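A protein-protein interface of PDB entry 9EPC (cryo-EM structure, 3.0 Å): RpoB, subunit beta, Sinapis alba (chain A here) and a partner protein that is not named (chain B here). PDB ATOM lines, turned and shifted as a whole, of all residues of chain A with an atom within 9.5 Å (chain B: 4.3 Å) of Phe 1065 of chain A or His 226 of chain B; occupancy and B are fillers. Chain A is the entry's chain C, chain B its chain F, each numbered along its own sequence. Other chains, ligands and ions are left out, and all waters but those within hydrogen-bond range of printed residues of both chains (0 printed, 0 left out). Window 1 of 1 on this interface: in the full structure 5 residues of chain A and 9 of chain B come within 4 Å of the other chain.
Printed residues of chain B within 4 Å of Glu 1062 of chain A: His 226 (3.0 Å) and Leu 230 (3.2 Å).
Printed residues of chain B within 4 Å of Lys 1063 of chain A: His 226 (2.5 Å) and Ser 227 (3.2 Å).
Of chain B, only His 226, Val 254, Gln 255, Cys 258 and Val 263 come within 4 Å of Phe 1065 of chain A.
Ile 1067 of chain A touches none of the printed residues of chain B.
Gly 224 of chain B touches none of the printed residues of chain A.
His 226 of chain B touches three residues of chain A.
Ser 227 of chain B touches just one residue of chain A: Lys 1063 (3.2 Å).
No residue of chain A comes within 4 Å of Ala 229 of chain B.
Leu 251 of chain B touches none of the printed residues of chain A.
Of the printed residues of chain A, Cys 258 of chain B touches Phe 1065.
The nearest printed residue of chain B that does not touch Phe 1065 of chain A is Leu 251 of chain B (5.5 Å).
The nearest residue of chain A that does not touch His 226 of chain B is Asn 1064 of chain A (4.6 Å).
Of the 12 printed residues of chain B, 7 touch a printed residue of chain A.
Printed residues of chain B that touch a printed residue of chain A: His 226, Ser 227, Leu 230, Val 254, Gln 255, Cys 258 and Val 263.
Printed residues of chain A that touch a printed residue of chain B: Val 1060, Glu 1062, Lys 1063 and Phe 1065.
Among the printed residues, no Asp or Glu carboxylate lies within 4 Å of a Lys or Arg side-chain nitrogen of the other chain.
The backbone carbonyl oxygen (O) of Lys 1063 of chain A sits at hydrogen-bond distance from a ring nitrogen (ND1) of His 226 of chain B (2.5 Å).
The backbone NH of Ser 227 of chain B is in hydrogen-bond range of the backbone carbonyl oxygen of Lys 1063 of chain A.
The side-chain hydroxyl (OG) of Ser 1061 of chain A sits at hydrogen-bond distance from the backbone NH (N) of Lys 1063 of chain A.
The side-chain carboxylate of Asp 225 of chain B is in hydrogen-bond range of the side-chain hydroxyl of Ser 227 of chain B (3.3 Å).
NE2 of His 226 of chain B lies within hydrogen-bond range of NE2 of Gln 255 of chain B (3.1 Å).
The side-chain hydroxyl (OG) of Ser 227 of chain B is in hydrogen-bond range of the side-chain amide nitrogen (ND2) of Asn 228 of chain B.
O of Gln 255 of chain B lies within hydrogen-bond range of SG of Cys 258 of chain B, at 3.2 Å.
The side-chain amide oxygen (OE1) of Gln 255 of chain B sits close to the backbone carbonyl oxygen (O) of Val 263 of chain B, at 3.1 Å.
Among the printed residues, pairs that only touch across the chains: Val 1060 of chain A with Val 263 of chain B, Glu 1062 of chain A with His 226 of chain B, Glu 1062 of chain A with Leu 230 of chain B, Phe 1065 of chain A with His 226 of chain B, Phe 1065 of chain A with Val 254 of chain B, Phe 1065 of chain A with Gln 255 of chain B, Phe 1065 of chain A with Cys 258 of chain B and Phe 1065 of chain A with Val 263 of chain B.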
ATOM      1  N   LEU A1059      -0.038 -17.582   5.341  1.00  0.00           N
ATOM      2  CA  LEU A1059       0.613 -18.000   6.579  1.00  0.00           C
ATOM      3  C   LEU A1059       1.617 -16.917   6.954  1.00  0.00           C
ATOM      4  O   LEU A1059       2.791 -16.993   6.586  1.00  0.00           O
ATOM      5  CB  LEU A1059       1.298 -19.350   6.429  1.00  0.00           C
ATOM      6  CG  LEU A1059       0.445 -20.559   6.054  1.00  0.00           C
ATOM      7  CD1 LEU A1059       1.246 -21.831   6.271  1.00  0.00           C
ATOM      8  CD2 LEU A1059      -0.836 -20.583   6.860  1.00  0.00           C
ATOM      9  N   VAL A1060       1.155 -15.906   7.685  1.00  0.00           N
ATOM     10  CA  VAL A1060       2.063 -14.884   8.188  1.00  0.00           C
ATOM     11  C   VAL A1060       2.979 -15.525   9.223  1.00  0.00           C
ATOM     12  O   VAL A1060       2.517 -16.057  10.239  1.00  0.00           O
ATOM     13  CB  VAL A1060       1.289 -13.697   8.771  1.00  0.00           C
ATOM     14  CG1 VAL A1060      -0.202 -13.936   8.662  1.00  0.00           C
ATOM     15  CG2 VAL A1060       1.690 -13.459  10.219  1.00  0.00           C
ATOM     16  N   SER A1061       4.280 -15.493   8.955  1.00  0.00           N
ATOM     17  CA  SER A1061       5.241 -16.177   9.806  1.00  0.00           C
ATOM     18  C   SER A1061       5.313 -15.527  11.181  1.00  0.00           C
ATOM     19  O   SER A1061       5.173 -14.311  11.332  1.00  0.00           O
ATOM     20  CB  SER A1061       6.625 -16.174   9.158  1.00  0.00           C
ATOM     21  OG  SER A1061       7.587 -16.760  10.016  1.00  0.00           O
ATOM     22  N   GLU A1062       5.526 -16.360  12.195  1.00  0.00           N
ATOM     23  CA  GLU A1062       5.708 -15.883  13.557  1.00  0.00           C
ATOM     24  C   GLU A1062       7.154 -15.529  13.868  1.00  0.00           C
ATOM     25  O   GLU A1062       7.426 -15.000  14.949  1.00  0.00           O
ATOM     26  CB  GLU A1062       5.219 -16.933  14.561  1.00  0.00           C
ATOM     27  CG  GLU A1062       6.061 -18.202  14.610  1.00  0.00           C
ATOM     28  CD  GLU A1062       5.822 -19.120  13.425  1.00  0.00           C
ATOM     29  OE1 GLU A1062       4.859 -18.879  12.667  1.00  0.00           O
ATOM     30  OE2 GLU A1062       6.596 -20.084  13.252  1.00  0.00           O
ATOM     31  N   LYS A1063       8.081 -15.802  12.950  1.00  0.00           N
ATOM     32  CA  LYS A1063       9.498 -15.540  13.181  1.00  0.00           C
ATOM     33  C   LYS A1063       9.902 -14.161  12.669  1.00  0.00           C
ATOM     34  O   LYS A1063      10.375 -13.319  13.438  1.00  0.00           O
ATOM     35  CB  LYS A1063      10.343 -16.629  12.513  1.00  0.00           C
ATOM     36  CG  LYS A1063       9.914 -18.043  12.856  1.00  0.00           C
ATOM     37  CD  LYS A1063      10.205 -18.372  14.307  1.00  0.00           C
ATOM     38  CE  LYS A1063      11.698 -18.342  14.583  1.00  0.00           C
ATOM     39  NZ  LYS A1063      12.006 -18.724  15.987  1.00  0.00           N
ATOM     40  N   ASN A1064       9.715 -13.917  11.371  1.00  0.00           N
ATOM     41  CA  ASN A1064      10.096 -12.653  10.748  1.00  0.00           C
ATOM     42  C   ASN A1064       8.922 -11.973  10.057  1.00  0.00           C
ATOM     43  O   ASN A1064       9.129 -11.089   9.220  1.00  0.00           O
ATOM     44  CB  ASN A1064      11.240 -12.871   9.758  1.00  0.00           C
ATOM     45  CG  ASN A1064      10.974 -14.020   8.810  1.00  0.00           C
ATOM     46  OD1 ASN A1064       9.852 -14.514   8.715  1.00  0.00           O
ATOM     47  ND2 ASN A1064      12.010 -14.454   8.104  1.00  0.00           N
ATOM     48  N   PHE A1065       7.692 -12.375  10.386  1.00  0.00           N
ATOM     49  CA  PHE A1065       6.477 -11.769   9.839  1.00  0.00           C
ATOM     50  C   PHE A1065       6.435 -11.859   8.316  1.00  0.00           C
ATOM     51  O   PHE A1065       5.906 -10.971   7.644  1.00  0.00           O
ATOM     52  CB  PHE A1065       6.330 -10.316  10.295  1.00  0.00           C
ATOM     53  CG  PHE A1065       6.851 -10.066  11.679  1.00  0.00           C
ATOM     54  CD1 PHE A1065       6.218 -10.611  12.781  1.00  0.00           C
ATOM     55  CD2 PHE A1065       7.978  -9.288  11.878  1.00  0.00           C
ATOM     56  CE1 PHE A1065       6.699 -10.384  14.055  1.00  0.00           C
ATOM     57  CE2 PHE A1065       8.461  -9.057  13.150  1.00  0.00           C
ATOM     58  CZ  PHE A1065       7.821  -9.605  14.238  1.00  0.00           C
ATOM     59  N   GLN A1066       6.983 -12.938   7.764  1.00  0.00           N
ATOM     60  CA  GLN A1066       7.030 -13.133   6.320  1.00  0.00           C
ATOM     61  C   GLN A1066       5.713 -13.747   5.865  1.00  0.00           C
ATOM     62  O   GLN A1066       5.402 -14.892   6.209  1.00  0.00           O
ATOM     63  CB  GLN A1066       8.210 -14.024   5.944  1.00  0.00           C
ATOM     64  CG  GLN A1066       8.526 -14.054   4.461  1.00  0.00           C
ATOM     65  CD  GLN A1066       9.201 -12.784   3.985  1.00  0.00           C
ATOM     66  OE1 GLN A1066       9.637 -11.960   4.790  1.00  0.00           O
ATOM     67  NE2 GLN A1066       9.294 -12.620   2.671  1.00  0.00           N
ATOM     68  N   ILE A1067       4.939 -12.993   5.092  1.00  0.00           N
ATOM     69  CA  ILE A1067       3.655 -13.474   4.593  1.00  0.00           C
ATOM     70  C   ILE A1067       3.895 -14.306   3.341  1.00  0.00           C
ATOM     71  O   ILE A1067       4.488 -13.828   2.369  1.00  0.00           O
ATOM     72  CB  ILE A1067       2.702 -12.308   4.300  1.00  0.00           C
ATOM     73  CG1 ILE A1067       2.428 -11.505   5.571  1.00  0.00           C
ATOM     74  CG2 ILE A1067       1.403 -12.823   3.705  1.00  0.00           C
ATOM     75  CD1 ILE A1067       1.479 -10.351   5.354  1.00  0.00           C
ATOM     76  N   ASN A1068       3.432 -15.552   3.360  1.00  0.00           N
ATOM     77  CA  ASN A1068       3.505 -16.426   2.199  1.00  0.00           C
ATOM     78  C   ASN A1068       2.116 -16.966   1.897  1.00  0.00           C
ATOM     79  O   ASN A1068       1.372 -17.339   2.807  1.00  0.00           O
ATOM     80  CB  ASN A1068       4.490 -17.581   2.420  1.00  0.00           C
ATOM     81  CG  ASN A1068       4.095 -18.471   3.577  1.00  0.00           C
ATOM     82  OD1 ASN A1068       3.377 -19.456   3.401  1.00  0.00           O
ATOM     83  ND2 ASN A1068       4.565 -18.134   4.771  1.00  0.00           N
ATOM     84  N   GLY B 224      16.432  -5.530  15.129  1.00  0.00           N
ATOM     85  CA  GLY B 224      15.380  -6.088  14.299  1.00  0.00           C
ATOM     86  C   GLY B 224      15.569  -7.555  13.983  1.00  0.00           C
ATOM     87  O   GLY B 224      15.346  -7.974  12.840  1.00  0.00           O
ATOM     88  N   ASP B 225      15.971  -8.350  14.973  1.00  0.00           N
ATOM     89  CA  ASP B 225      16.244  -9.767  14.767  1.00  0.00           C
ATOM     90  C   ASP B 225      15.243 -10.602  15.550  1.00  0.00           C
ATOM     91  O   ASP B 225      15.621 -11.548  16.249  1.00  0.00           O
ATOM     92  CB  ASP B 225      17.678 -10.103  15.178  1.00  0.00           C
ATOM     93  CG  ASP B 225      18.143 -11.437  14.631  1.00  0.00           C
ATOM     94  OD1 ASP B 225      17.363 -12.087  13.903  1.00  0.00           O
ATOM     95  OD2 ASP B 225      19.287 -11.837  14.930  1.00  0.00           O
ATOM     96  N   HIS B 226      13.962 -10.236  15.450  1.00  0.00           N
ATOM     97  CA  HIS B 226      12.916 -10.920  16.205  1.00  0.00           C
ATOM     98  C   HIS B 226      12.902 -12.419  15.939  1.00  0.00           C
ATOM     99  O   HIS B 226      12.551 -13.200  16.831  1.00  0.00           O
ATOM    100  CB  HIS B 226      11.556 -10.310  15.868  1.00  0.00           C
ATOM    101  CG  HIS B 226      10.395 -11.129  16.334  1.00  0.00           C
ATOM    102  ND1 HIS B 226       9.710 -11.986  15.502  1.00  0.00           N
ATOM    103  CD2 HIS B 226       9.801 -11.226  17.546  1.00  0.00           C
ATOM    104  CE1 HIS B 226       8.741 -12.574  16.180  1.00  0.00           C
ATOM    105  NE2 HIS B 226       8.775 -12.130  17.423  1.00  0.00           N
ATOM    106  N   SER B 227      13.278 -12.840  14.730  1.00  0.00           N
ATOM    107  CA  SER B 227      13.312 -14.267  14.427  1.00  0.00           C
ATOM    108  C   SER B 227      14.287 -14.999  15.339  1.00  0.00           C
ATOM    109  O   SER B 227      13.967 -16.066  15.875  1.00  0.00           O
ATOM    110  CB  SER B 227      13.682 -14.482  12.962  1.00  0.00           C
ATOM    111  OG  SER B 227      14.956 -13.928  12.676  1.00  0.00           O
ATOM    112  N   ASN B 228      15.481 -14.440  15.531  1.00  0.00           N
ATOM    113  CA  ASN B 228      16.439 -15.048  16.445  1.00  0.00           C
ATOM    114  C   ASN B 228      16.058 -14.801  17.899  1.00  0.00           C
ATOM    115  O   ASN B 228      16.245 -15.679  18.748  1.00  0.00           O
ATOM    116  CB  ASN B 228      17.844 -14.520  16.164  1.00  0.00           C
ATOM    117  CG  ASN B 228      18.403 -15.028  14.852  1.00  0.00           C
ATOM    118  OD1 ASN B 228      19.210 -15.956  14.827  1.00  0.00           O
ATOM    119  ND2 ASN B 228      17.969 -14.427  13.751  1.00  0.00           N
ATOM    120  N   ALA B 229      15.525 -13.616  18.203  1.00  0.00           N
ATOM    121  CA  ALA B 229      15.132 -13.316  19.575  1.00  0.00           C
ATOM    122  C   ALA B 229      14.022 -14.244  20.047  1.00  0.00           C
ATOM    123  O   ALA B 229      14.064 -14.751  21.175  1.00  0.00           O
ATOM    124  CB  ALA B 229      14.696 -11.857  19.689  1.00  0.00           C
ATOM    125  N   LEU B 230      13.019 -14.481  19.199  1.00  0.00           N
ATOM    126  CA  LEU B 230      11.935 -15.382  19.576  1.00  0.00           C
ATOM    127  C   LEU B 230      12.445 -16.804  19.766  1.00  0.00           C
ATOM    128  O   LEU B 230      12.044 -17.495  20.709  1.00  0.00           O
ATOM    129  CB  LEU B 230      10.827 -15.345  18.527  1.00  0.00           C
ATOM    130  CG  LEU B 230       9.575 -16.145  18.879  1.00  0.00           C
ATOM    131  CD1 LEU B 230       8.916 -15.578  20.124  1.00  0.00           C
ATOM    132  CD2 LEU B 230       8.602 -16.159  17.718  1.00  0.00           C
ATOM    133  N   LEU B 251      10.247  -8.148  22.410  1.00  0.00           N
ATOM    134  CA  LEU B 251       9.637  -8.753  21.230  1.00  0.00           C
ATOM    135  C   LEU B 251       8.586  -7.837  20.616  1.00  0.00           C
ATOM    136  O   LEU B 251       8.479  -7.745  19.388  1.00  0.00           O
ATOM    137  CB  LEU B 251       9.023 -10.104  21.590  1.00  0.00           C
ATOM    138  CG  LEU B 251       9.965 -11.151  22.183  1.00  0.00           C
ATOM    139  CD1 LEU B 251       9.244 -12.476  22.346  1.00  0.00           C
ATOM    140  CD2 LEU B 251      11.201 -11.314  21.319  1.00  0.00           C
ATOM    141  N   VAL B 254       9.520  -5.085  17.997  1.00  0.00           N
ATOM    142  CA  VAL B 254       9.684  -5.459  16.602  1.00  0.00           C
ATOM    143  C   VAL B 254       8.354  -5.829  15.960  1.00  0.00           C
ATOM    144  O   VAL B 254       8.108  -5.492  14.802  1.00  0.00           O
ATOM    145  CB  VAL B 254      10.701  -6.613  16.479  1.00  0.00           C
ATOM    146  CG1 VAL B 254      11.062  -6.844  15.023  1.00  0.00           C
ATOM    147  CG2 VAL B 254      11.938  -6.315  17.303  1.00  0.00           C
ATOM    148  N   GLN B 255       7.487  -6.523  16.700  1.00  0.00           N
ATOM    149  CA  GLN B 255       6.193  -6.914  16.153  1.00  0.00           C
ATOM    150  C   GLN B 255       5.311  -5.708  15.866  1.00  0.00           C
ATOM    151  O   GLN B 255       4.460  -5.764  14.972  1.00  0.00           O
ATOM    152  CB  GLN B 255       5.483  -7.866  17.114  1.00  0.00           C
ATOM    153  CG  GLN B 255       6.273  -9.115  17.440  1.00  0.00           C
ATOM    154  CD  GLN B 255       5.589  -9.971  18.479  1.00  0.00           C
ATOM    155  OE1 GLN B 255       4.440  -9.728  18.840  1.00  0.00           O
ATOM    156  NE2 GLN B 255       6.296 -10.980  18.971  1.00  0.00           N
ATOM    157  N   CYS B 258       5.702  -4.606  12.173  1.00  0.00           N
ATOM    158  CA  CYS B 258       5.457  -5.522  11.067  1.00  0.00           C
ATOM    159  C   CYS B 258       4.256  -5.121  10.222  1.00  0.00           C
ATOM    160  O   CYS B 258       4.093  -5.653   9.120  1.00  0.00           O
ATOM    161  CB  CYS B 258       5.257  -6.943  11.592  1.00  0.00           C
ATOM    162  SG  CYS B 258       3.634  -7.250  12.318  1.00  0.00           S
ATOM    163  N   VAL B 263      -0.363  -9.866  15.067  1.00  0.00           N
ATOM    164  CA  VAL B 263       0.872 -10.486  15.536  1.00  0.00           C
ATOM    165  C   VAL B 263       1.275  -9.903  16.884  1.00  0.00           C
ATOM    166  O   VAL B 263       1.634 -10.633  17.815  1.00  0.00           O
ATOM    167  CB  VAL B 263       1.988 -10.315  14.491  1.00  0.00           C
ATOM    168  CG1 VAL B 263       3.295 -10.867  15.022  1.00  0.00           C
ATOM    169  CG2 VAL B 263       1.601 -11.004  13.194  1.00  0.00           C
